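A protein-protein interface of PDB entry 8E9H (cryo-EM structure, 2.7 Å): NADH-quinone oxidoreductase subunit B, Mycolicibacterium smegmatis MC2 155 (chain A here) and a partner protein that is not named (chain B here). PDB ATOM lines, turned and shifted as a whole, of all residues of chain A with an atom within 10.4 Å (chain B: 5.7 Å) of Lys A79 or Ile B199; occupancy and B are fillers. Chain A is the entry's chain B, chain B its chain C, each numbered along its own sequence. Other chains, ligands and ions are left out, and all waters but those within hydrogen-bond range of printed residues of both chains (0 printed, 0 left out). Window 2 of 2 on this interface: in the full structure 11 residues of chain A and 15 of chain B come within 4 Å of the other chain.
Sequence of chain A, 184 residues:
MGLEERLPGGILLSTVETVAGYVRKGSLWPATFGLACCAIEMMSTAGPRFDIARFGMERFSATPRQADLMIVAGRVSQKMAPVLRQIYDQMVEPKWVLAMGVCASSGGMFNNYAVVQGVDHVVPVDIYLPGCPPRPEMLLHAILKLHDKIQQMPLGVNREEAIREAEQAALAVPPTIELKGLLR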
ATOM      1  N   PHE A  33      14.872  -3.421  -4.725  1.00  0.00           N
ATOM      2  CA  PHE A  33      15.535  -2.172  -4.382  1.00  0.00           C
ATOM      3  C   PHE A  33      14.869  -0.975  -5.046  1.00  0.00           C
ATOM      4  O   PHE A  33      15.541  -0.146  -5.664  1.00  0.00           O
ATOM      5  CB  PHE A  33      17.007  -2.250  -4.779  1.00  0.00           C
ATOM      6  CG  PHE A  33      17.806  -1.059  -4.366  1.00  0.00           C
ATOM      7  CD1 PHE A  33      17.948  -0.735  -3.033  1.00  0.00           C
ATOM      8  CD2 PHE A  33      18.416  -0.263  -5.312  1.00  0.00           C
ATOM      9  CE1 PHE A  33      18.682   0.358  -2.652  1.00  0.00           C
ATOM     10  CE2 PHE A  33      19.150   0.831  -4.937  1.00  0.00           C
ATOM     11  CZ  PHE A  33      19.287   1.142  -3.607  1.00  0.00           C
ATOM     12  N   LEU A  35      13.144   2.635  -5.440  1.00  0.00           N
ATOM     13  CA  LEU A  35      13.267   3.959  -4.853  1.00  0.00           C
ATOM     14  C   LEU A  35      12.224   4.874  -5.472  1.00  0.00           C
ATOM     15  O   LEU A  35      11.842   4.695  -6.632  1.00  0.00           O
ATOM     16  CB  LEU A  35      14.656   4.551  -5.094  1.00  0.00           C
ATOM     17  CG  LEU A  35      15.798   4.152  -4.167  1.00  0.00           C
ATOM     18  CD1 LEU A  35      15.925   2.652  -4.087  1.00  0.00           C
ATOM     19  CD2 LEU A  35      17.094   4.768  -4.648  1.00  0.00           C
ATOM     20  N   ARG A  75      15.042   8.014  -7.637  1.00  0.00           N
ATOM     21  CA  ARG A  75      16.024   9.066  -7.442  1.00  0.00           C
ATOM     22  C   ARG A  75      16.914   8.757  -6.250  1.00  0.00           C
ATOM     23  O   ARG A  75      16.429   8.456  -5.157  1.00  0.00           O
ATOM     24  CB  ARG A  75      15.313  10.407  -7.276  1.00  0.00           C
ATOM     25  CG  ARG A  75      14.412  10.516  -6.075  1.00  0.00           C
ATOM     26  CD  ARG A  75      13.697  11.846  -6.119  1.00  0.00           C
ATOM     27  NE  ARG A  75      12.812  12.068  -4.983  1.00  0.00           N
ATOM     28  CZ  ARG A  75      11.537  11.707  -4.946  1.00  0.00           C
ATOM     29  NH1 ARG A  75      10.953  11.125  -5.979  1.00  0.00           N
ATOM     30  NH2 ARG A  75      10.825  11.951  -3.850  1.00  0.00           N
ATOM     31  N   VAL A  76      18.223   8.821  -6.472  1.00  0.00           N
ATOM     32  CA  VAL A  76      19.212   8.476  -5.460  1.00  0.00           C
ATOM     33  C   VAL A  76      19.629   9.756  -4.753  1.00  0.00           C
ATOM     34  O   VAL A  76      20.323  10.596  -5.328  1.00  0.00           O
ATOM     35  CB  VAL A  76      20.422   7.773  -6.080  1.00  0.00           C
ATOM     36  CG1 VAL A  76      21.399   7.352  -5.004  1.00  0.00           C
ATOM     37  CG2 VAL A  76      19.978   6.575  -6.886  1.00  0.00           C
ATOM     38  N   SER A  77      19.208   9.904  -3.504  1.00  0.00           N
ATOM     39  CA  SER A  77      19.625  11.044  -2.711  1.00  0.00           C
ATOM     40  C   SER A  77      21.075  10.881  -2.276  1.00  0.00           C
ATOM     41  O   SER A  77      21.658   9.798  -2.352  1.00  0.00           O
ATOM     42  CB  SER A  77      18.728  11.197  -1.489  1.00  0.00           C
ATOM     43  OG  SER A  77      18.981  10.167  -0.553  1.00  0.00           O
ATOM     44  N   GLN A  78      21.664  11.983  -1.816  1.00  0.00           N
ATOM     45  CA  GLN A  78      23.055  11.943  -1.379  1.00  0.00           C
ATOM     46  C   GLN A  78      23.243  10.920  -0.271  1.00  0.00           C
ATOM     47  O   GLN A  78      24.158  10.092  -0.321  1.00  0.00           O
ATOM     48  CB  GLN A  78      23.495  13.327  -0.909  1.00  0.00           C
ATOM     49  CG  GLN A  78      23.552  14.365  -2.009  1.00  0.00           C
ATOM     50  CD  GLN A  78      24.831  14.295  -2.804  1.00  0.00           C
ATOM     51  OE1 GLN A  78      25.609  13.356  -2.666  1.00  0.00           O
ATOM     52  NE2 GLN A  78      25.060  15.294  -3.643  1.00  0.00           N
ATOM     53  N   LYS A  79      22.373  10.952   0.737  1.00  0.00           N
ATOM     54  CA  LYS A  79      22.512  10.029   1.854  1.00  0.00           C
ATOM     55  C   LYS A  79      22.327   8.583   1.427  1.00  0.00           C
ATOM     56  O   LYS A  79      22.766   7.678   2.141  1.00  0.00           O
ATOM     57  CB  LYS A  79      21.507  10.372   2.951  1.00  0.00           C
ATOM     58  CG  LYS A  79      21.898   9.826   4.306  1.00  0.00           C
ATOM     59  CD  LYS A  79      21.339  10.649   5.448  1.00  0.00           C
ATOM     60  CE  LYS A  79      19.863  10.399   5.643  1.00  0.00           C
ATOM     61  NZ  LYS A  79      19.330  11.174   6.792  1.00  0.00           N
ATOM     62  N   MET A  80      21.694   8.344   0.283  1.00  0.00           N
ATOM     63  CA  MET A  80      21.395   6.989  -0.149  1.00  0.00           C
ATOM     64  C   MET A  80      22.479   6.396  -1.032  1.00  0.00           C
ATOM     65  O   MET A  80      22.569   5.169  -1.136  1.00  0.00           O
ATOM     66  CB  MET A  80      20.064   6.969  -0.901  1.00  0.00           C
ATOM     67  CG  MET A  80      19.648   5.612  -1.412  1.00  0.00           C
ATOM     68  SD  MET A  80      19.292   4.500  -0.049  1.00  0.00           S
ATOM     69  CE  MET A  80      18.416   3.210  -0.909  1.00  0.00           C
ATOM     70  N   ALA A  81      23.298   7.228  -1.665  1.00  0.00           N
ATOM     71  CA  ALA A  81      24.339   6.701  -2.537  1.00  0.00           C
ATOM     72  C   ALA A  81      25.219   5.673  -1.844  1.00  0.00           C
ATOM     73  O   ALA A  81      25.486   4.621  -2.450  1.00  0.00           O
ATOM     74  CB  ALA A  81      25.181   7.857  -3.081  1.00  0.00           C
ATOM     75  N   PRO A  82      25.712   5.898  -0.626  1.00  0.00           N
ATOM     76  CA  PRO A  82      26.485   4.841   0.038  1.00  0.00           C
ATOM     77  C   PRO A  82      25.710   3.548   0.187  1.00  0.00           C
ATOM     78  O   PRO A  82      26.271   2.466  -0.013  1.00  0.00           O
ATOM     79  CB  PRO A  82      26.821   5.467   1.395  1.00  0.00           C
ATOM     80  CG  PRO A  82      26.786   6.923   1.146  1.00  0.00           C
ATOM     81  CD  PRO A  82      25.667   7.124   0.182  1.00  0.00           C
ATOM     82  N   VAL A  83      24.423   3.631   0.516  1.00  0.00           N
ATOM     83  CA  VAL A  83      23.615   2.427   0.663  1.00  0.00           C
ATOM     84  C   VAL A  83      23.476   1.715  -0.674  1.00  0.00           C
ATOM     85  O   VAL A  83      23.574   0.486  -0.757  1.00  0.00           O
ATOM     86  CB  VAL A  83      22.240   2.778   1.255  1.00  0.00           C
ATOM     87  CG1 VAL A  83      21.403   1.532   1.419  1.00  0.00           C
ATOM     88  CG2 VAL A  83      22.405   3.488   2.579  1.00  0.00           C
ATOM     89  N   LEU A  84      23.225   2.474  -1.737  1.00  0.00           N
ATOM     90  CA  LEU A  84      23.080   1.865  -3.052  1.00  0.00           C
ATOM     91  C   LEU A  84      24.371   1.185  -3.478  1.00  0.00           C
ATOM     92  O   LEU A  84      24.348   0.077  -4.024  1.00  0.00           O
ATOM     93  CB  LEU A  84      22.665   2.924  -4.067  1.00  0.00           C
ATOM     94  CG  LEU A  84      22.238   2.410  -5.436  1.00  0.00           C
ATOM     95  CD1 LEU A  84      21.157   3.302  -6.000  1.00  0.00           C
ATOM     96  CD2 LEU A  84      23.417   2.346  -6.385  1.00  0.00           C
ATOM     97  N   ARG A  85      25.511   1.832  -3.238  1.00  0.00           N
ATOM     98  CA  ARG A  85      26.784   1.209  -3.578  1.00  0.00           C
ATOM     99  C   ARG A  85      27.016  -0.040  -2.746  1.00  0.00           C
ATOM    100  O   ARG A  85      27.549  -1.034  -3.246  1.00  0.00           O
ATOM    101  CB  ARG A  85      27.931   2.195  -3.381  1.00  0.00           C
ATOM    102  CG  ARG A  85      29.302   1.609  -3.686  1.00  0.00           C
ATOM    103  CD  ARG A  85      29.531   1.476  -5.170  1.00  0.00           C
ATOM    104  NE  ARG A  85      30.378   0.334  -5.486  1.00  0.00           N
ATOM    105  CZ  ARG A  85      30.979   0.148  -6.652  1.00  0.00           C
ATOM    106  NH1 ARG A  85      30.848   1.013  -7.643  1.00  0.00           N
ATOM    107  NH2 ARG A  85      31.728  -0.934  -6.830  1.00  0.00           N
ATOM    108  N   GLN A  86      26.647  -0.005  -1.466  1.00  0.00           N
ATOM    109  CA  GLN A  86      26.798  -1.193  -0.637  1.00  0.00           C
ATOM    110  C   GLN A  86      25.965  -2.341  -1.182  1.00  0.00           C
ATOM    111  O   GLN A  86      26.431  -3.482  -1.248  1.00  0.00           O
ATOM    112  CB  GLN A  86      26.401  -0.885   0.803  1.00  0.00           C
ATOM    113  CG  GLN A  86      26.652  -2.028   1.760  1.00  0.00           C
ATOM    114  CD  GLN A  86      28.120  -2.276   1.987  1.00  0.00           C
ATOM    115  OE1 GLN A  86      28.969  -1.555   1.469  1.00  0.00           O
ATOM    116  NE2 GLN A  86      28.430  -3.303   2.761  1.00  0.00           N
ATOM    117  N   ASN A 112      19.861  19.423  -8.258  1.00  0.00           N
ATOM    118  CA  ASN A 112      20.138  20.184  -7.051  1.00  0.00           C
ATOM    119  C   ASN A 112      21.075  19.394  -6.149  1.00  0.00           C
ATOM    120  O   ASN A 112      21.554  18.315  -6.501  1.00  0.00           O
ATOM    121  CB  ASN A 112      18.844  20.534  -6.314  1.00  0.00           C
ATOM    122  CG  ASN A 112      18.080  19.312  -5.876  1.00  0.00           C
ATOM    123  OD1 ASN A 112      18.612  18.208  -5.857  1.00  0.00           O
ATOM    124  ND2 ASN A 112      16.819  19.501  -5.529  1.00  0.00           N
ATOM    125  N   TYR A 113      21.317  19.953  -4.964  1.00  0.00           N
ATOM    126  CA  TYR A 113      22.285  19.379  -4.035  1.00  0.00           C
ATOM    127  C   TYR A 113      21.911  17.964  -3.618  1.00  0.00           C
ATOM    128  O   TYR A 113      22.774  17.085  -3.526  1.00  0.00           O
ATOM    129  CB  TYR A 113      22.390  20.268  -2.797  1.00  0.00           C
ATOM    130  CG  TYR A 113      21.101  20.330  -2.020  1.00  0.00           C
ATOM    131  CD1 TYR A 113      20.065  21.153  -2.423  1.00  0.00           C
ATOM    132  CD2 TYR A 113      20.906  19.542  -0.901  1.00  0.00           C
ATOM    133  CE1 TYR A 113      18.882  21.200  -1.729  1.00  0.00           C
ATOM    134  CE2 TYR A 113      19.727  19.583  -0.202  1.00  0.00           C
ATOM    135  CZ  TYR A 113      18.716  20.409  -0.624  1.00  0.00           C
ATOM    136  OH  TYR A 113      17.538  20.454   0.077  1.00  0.00           O
ATOM    137  N   ALA A 114      20.628  17.724  -3.347  1.00  0.00           N
ATOM    138  CA  ALA A 114      20.228  16.521  -2.631  1.00  0.00           C
ATOM    139  C   ALA A 114      20.333  15.259  -3.471  1.00  0.00           C
ATOM    140  O   ALA A 114      20.463  14.171  -2.906  1.00  0.00           O
ATOM    141  CB  ALA A 114      18.796  16.667  -2.126  1.00  0.00           C
ATOM    142  N   VAL A 115      20.270  15.367  -4.792  1.00  0.00           N
ATOM    143  CA  VAL A 115      20.232  14.206  -5.670  1.00  0.00           C
ATOM    144  C   VAL A 115      21.612  14.009  -6.275  1.00  0.00           C
ATOM    145  O   VAL A 115      22.359  14.973  -6.467  1.00  0.00           O
ATOM    146  CB  VAL A 115      19.167  14.363  -6.771  1.00  0.00           C
ATOM    147  CG1 VAL A 115      19.084  13.109  -7.608  1.00  0.00           C
ATOM    148  CG2 VAL A 115      17.827  14.675  -6.155  1.00  0.00           C
ATOM    149  N   VAL A 116      21.946  12.751  -6.578  1.00  0.00           N
ATOM    150  CA  VAL A 116      23.294  12.399  -7.019  1.00  0.00           C
ATOM    151  C   VAL A 116      23.555  12.741  -8.475  1.00  0.00           C
ATOM    152  O   VAL A 116      24.711  12.698  -8.910  1.00  0.00           O
ATOM    153  CB  VAL A 116      23.537  10.897  -6.775  1.00  0.00           C
ATOM    154  CG1 VAL A 116      24.855  10.455  -7.370  1.00  0.00           C
ATOM    155  CG2 VAL A 116      23.514  10.602  -5.295  1.00  0.00           C
ATOM    156  N   GLN A 117      22.527  13.097  -9.239  1.00  0.00           N
ATOM    157  CA  GLN A 117      22.691  13.433 -10.653  1.00  0.00           C
ATOM    158  C   GLN A 117      23.170  12.225 -11.447  1.00  0.00           C
ATOM    159  O   GLN A 117      24.165  12.287 -12.170  1.00  0.00           O
ATOM    160  CB  GLN A 117      23.646  14.613 -10.838  1.00  0.00           C
ATOM    161  CG  GLN A 117      23.209  15.869 -10.125  1.00  0.00           C
ATOM    162  CD  GLN A 117      21.763  16.206 -10.395  1.00  0.00           C
ATOM    163  OE1 GLN A 117      21.352  16.336 -11.545  1.00  0.00           O
ATOM    164  NE2 GLN A 117      20.980  16.334  -9.336  1.00  0.00           N
ATOM    165  N   VAL A 122      27.967   6.384  -8.850  1.00  0.00           N
ATOM    166  CA  VAL A 122      28.380   5.466  -7.793  1.00  0.00           C
ATOM    167  C   VAL A 122      28.447   4.016  -8.238  1.00  0.00           C
ATOM    168  O   VAL A 122      29.171   3.223  -7.612  1.00  0.00           O
ATOM    169  CB  VAL A 122      27.448   5.604  -6.573  1.00  0.00           C
ATOM    170  CG1 VAL A 122      27.518   7.008  -6.028  1.00  0.00           C
ATOM    171  CG2 VAL A 122      26.026   5.252  -6.945  1.00  0.00           C
ATOM    172  N   TRP B 177      11.050  16.045  14.872  1.00  0.00           N
ATOM    173  CA  TRP B 177      11.167  15.736  13.451  1.00  0.00           C
ATOM    174  C   TRP B 177      10.689  16.895  12.591  1.00  0.00           C
ATOM    175  O   TRP B 177      10.942  16.915  11.386  1.00  0.00           O
ATOM    176  CB  TRP B 177      10.373  14.492  13.055  1.00  0.00           C
ATOM    177  CG  TRP B 177      10.878  13.221  13.604  1.00  0.00           C
ATOM    178  CD1 TRP B 177      11.618  13.042  14.729  1.00  0.00           C
ATOM    179  CD2 TRP B 177      10.690  11.928  13.034  1.00  0.00           C
ATOM    180  NE1 TRP B 177      11.899  11.711  14.902  1.00  0.00           N
ATOM    181  CE2 TRP B 177      11.338  11.007  13.870  1.00  0.00           C
ATOM    182  CE3 TRP B 177      10.033  11.461  11.897  1.00  0.00           C
ATOM    183  CZ2 TRP B 177      11.347   9.645  13.604  1.00  0.00           C
ATOM    184  CZ3 TRP B 177      10.044  10.115  11.635  1.00  0.00           C
ATOM    185  CH2 TRP B 177      10.693   9.221  12.483  1.00  0.00           C
ATOM    186  N   ARG B 180      13.579  19.269  14.082  1.00  0.00           N
ATOM    187  CA  ARG B 180      14.802  18.710  13.518  1.00  0.00           C
ATOM    188  C   ARG B 180      14.920  19.023  12.034  1.00  0.00           C
ATOM    189  O   ARG B 180      15.989  19.423  11.562  1.00  0.00           O
ATOM    190  CB  ARG B 180      14.845  17.202  13.755  1.00  0.00           C
ATOM    191  CG  ARG B 180      15.236  16.824  15.168  1.00  0.00           C
ATOM    192  CD  ARG B 180      15.250  15.325  15.370  1.00  0.00           C
ATOM    193  NE  ARG B 180      16.216  14.663  14.505  1.00  0.00           N
ATOM    194  CZ  ARG B 180      16.157  13.387  14.155  1.00  0.00           C
ATOM    195  NH1 ARG B 180      15.205  12.588  14.606  1.00  0.00           N
ATOM    196  NH2 ARG B 180      17.079  12.897  13.332  1.00  0.00           N
ATOM    197  N   GLU B 181      13.835  18.851  11.281  1.00  0.00           N
ATOM    198  CA  GLU B 181      13.884  19.117   9.848  1.00  0.00           C
ATOM    199  C   GLU B 181      14.171  20.586   9.575  1.00  0.00           C
ATOM    200  O   GLU B 181      14.985  20.921   8.705  1.00  0.00           O
ATOM    201  CB  GLU B 181      12.567  18.693   9.201  1.00  0.00           C
ATOM    202  CG  GLU B 181      12.453  19.016   7.722  1.00  0.00           C
ATOM    203  CD  GLU B 181      11.026  18.949   7.225  1.00  0.00           C
ATOM    204  OE1 GLU B 181      10.120  19.421   7.943  1.00  0.00           O
ATOM    205  OE2 GLU B 181      10.808  18.430   6.112  1.00  0.00           O
ATOM    206  N   ASP B 184      17.690  21.356  10.232  1.00  0.00           N
ATOM    207  CA  ASP B 184      18.533  20.833   9.167  1.00  0.00           C
ATOM    208  C   ASP B 184      18.527  21.765   7.968  1.00  0.00           C
ATOM    209  O   ASP B 184      19.575  22.050   7.380  1.00  0.00           O
ATOM    210  CB  ASP B 184      18.053  19.443   8.761  1.00  0.00           C
ATOM    211  CG  ASP B 184      19.078  18.693   7.946  1.00  0.00           C
ATOM    212  OD1 ASP B 184      20.135  19.279   7.642  1.00  0.00           O
ATOM    213  OD2 ASP B 184      18.826  17.521   7.603  1.00  0.00           O
ATOM    214  N   THR B 197      19.217  16.943  16.114  1.00  0.00           N
ATOM    215  CA  THR B 197      20.142  16.422  15.125  1.00  0.00           C
ATOM    216  C   THR B 197      19.523  16.486  13.734  1.00  0.00           C
ATOM    217  O   THR B 197      18.300  16.494  13.568  1.00  0.00           O
ATOM    218  CB  THR B 197      20.519  14.982  15.457  1.00  0.00           C
ATOM    219  OG1 THR B 197      19.356  14.153  15.375  1.00  0.00           O
ATOM    220  CG2 THR B 197      21.090  14.897  16.855  1.00  0.00           C
ATOM    221  N   ARG B 198      20.385  16.526  12.725  1.00  0.00           N
ATOM    222  CA  ARG B 198      19.911  16.511  11.353  1.00  0.00           C
ATOM    223  C   ARG B 198      19.117  15.239  11.087  1.00  0.00           C
ATOM    224  O   ARG B 198      19.441  14.157  11.580  1.00  0.00           O
ATOM    225  CB  ARG B 198      21.081  16.606  10.379  1.00  0.00           C
ATOM    226  CG  ARG B 198      21.734  17.966  10.340  1.00  0.00           C
ATOM    227  CD  ARG B 198      22.751  18.048   9.228  1.00  0.00           C
ATOM    228  NE  ARG B 198      23.468  19.316   9.241  1.00  0.00           N
ATOM    229  CZ  ARG B 198      23.170  20.360   8.480  1.00  0.00           C
ATOM    230  NH1 ARG B 198      22.165  20.330   7.622  1.00  0.00           N
ATOM    231  NH2 ARG B 198      23.899  21.465   8.584  1.00  0.00           N
ATOM    232  N   ILE B 199      18.060  15.380  10.294  1.00  0.00           N
ATOM    233  CA  ILE B 199      17.153  14.272  10.030  1.00  0.00           C
ATOM    234  C   ILE B 199      17.165  13.940   8.547  1.00  0.00           C
ATOM    235  O   ILE B 199      17.124  12.767   8.164  1.00  0.00           O
ATOM    236  CB  ILE B 199      15.731  14.594  10.522  1.00  0.00           C
ATOM    237  CG1 ILE B 199      14.799  13.420  10.241  1.00  0.00           C
ATOM    238  CG2 ILE B 199      15.203  15.851   9.866  1.00  0.00           C
ATOM    239  CD1 ILE B 199      13.527  13.465  11.040  1.00  0.00           C
ATOM    240  N   GLU B 200      17.221  14.965   7.700  1.00  0.00           N
ATOM    241  CA  GLU B 200      17.251  14.762   6.258  1.00  0.00           C
ATOM    242  C   GLU B 200      18.676  14.678   5.723  1.00  0.00           C
ATOM    243  O   GLU B 200      19.058  13.671   5.119  1.00  0.00           O
ATOM    244  CB  GLU B 200      16.492  15.893   5.562  1.00  0.00           C
ATOM    245  CG  GLU B 200      15.008  15.907   5.863  1.00  0.00           C
ATOM    246  CD  GLU B 200      14.258  14.816   5.148  1.00  0.00           C
ATOM    247  OE1 GLU B 200      14.902  14.022   4.438  1.00  0.00           O
ATOM    248  OE2 GLU B 200      13.021  14.755   5.291  1.00  0.00           O
ATOM    249  N   MET B 201      19.469  15.719   5.935  1.00  0.00           N
ATOM    250  CA  MET B 201      20.857  15.729   5.509  1.00  0.00           C
ATOM    251  C   MET B 201      21.712  14.810   6.370  1.00  0.00           C
ATOM    252  O   MET B 201      21.386  14.544   7.528  1.00  0.00           O
ATOM    253  CB  MET B 201      21.411  17.146   5.580  1.00  0.00           C
ATOM    254  CG  MET B 201      20.753  18.108   4.636  1.00  0.00           C
ATOM    255  SD  MET B 201      21.222  17.662   2.960  1.00  0.00           S
ATOM    256  CE  MET B 201      19.674  17.058   2.347  1.00  0.00           C
ATOM    257  N   PRO B 202      22.820  14.313   5.825  1.00  0.00           N
ATOM    258  CA  PRO B 202      23.781  13.597   6.663  1.00  0.00           C
ATOM    259  C   PRO B 202      24.294  14.498   7.771  1.00  0.00           C
ATOM    260  O   PRO B 202      24.451  15.707   7.596  1.00  0.00           O
ATOM    261  CB  PRO B 202      24.899  13.222   5.685  1.00  0.00           C
ATOM    262  CG  PRO B 202      24.267  13.258   4.355  1.00  0.00           C
ATOM    263  CD  PRO B 202      23.242  14.337   4.417  1.00  0.00           C
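The side-chain amino group (NZ) of Lys A79 lies within hydrogen-bond range of the backbone carbonyl oxygen (O) of Ile B199 (3.0 Å). O of Glu B200 is in hydrogen-bond range of NZ of Lys A79, at 3.0 Å.
O of Tyr A113 sits at hydrogen-bond distance from NE2 of Gln A78 (2.9 Å). OD2 of Asp B184 lies within hydrogen-bond range of N of Glu B200, 3.0 Å away. The backbone NH (N) of Met B201 lies within hydrogen-bond range of the side-chain carboxylate (OD2) of Asp B184 (2.5 Å).
Among the printed residues, pairs that only touch across the chains: Tyr A113 with Met B201 and Lys A79 with Pro B202.
Printed residues of chain B within 4 Å of Lys A79: Ile B199, Glu B200 and Pro B202. Printed residues of chain B within 4 Å of Tyr A113: Met B201 (3.6 Å). No residue of chain A comes within 4 Å of Arg B180. Thr B197 touches none of the printed residues of chain A. Ile B199 touches one residue of chain A. Of the printed residues of chain A, Met B201 touches Tyr A113 (3.6 Å). Pro B202 touches just one residue of chain A: Lys A79 (3.97 Å). The nearest printed residue of chain B that does not touch Lys A79 is Met B201 (4.02 Å). The nearest printed residue of chain B that does not touch Tyr A113 is Glu B200 (7.2 Å).
Hydrophobic or aromatic side chains of chain A within 4 Å of the printed part of chain B: Tyr A113. Of the 10 printed residues of chain B, 4 touch a printed residue of chain A. Printed residues of chain B that touch a printed residue of chain A: Ile B199, Glu B200, Met B201 and Pro B202. Among the printed residues, 4 pairs touch across the chains. Among the printed residues, no Asp or Glu carboxylate lies within 4 Å of a Lys or Arg side-chain nitrogen of the other chain.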
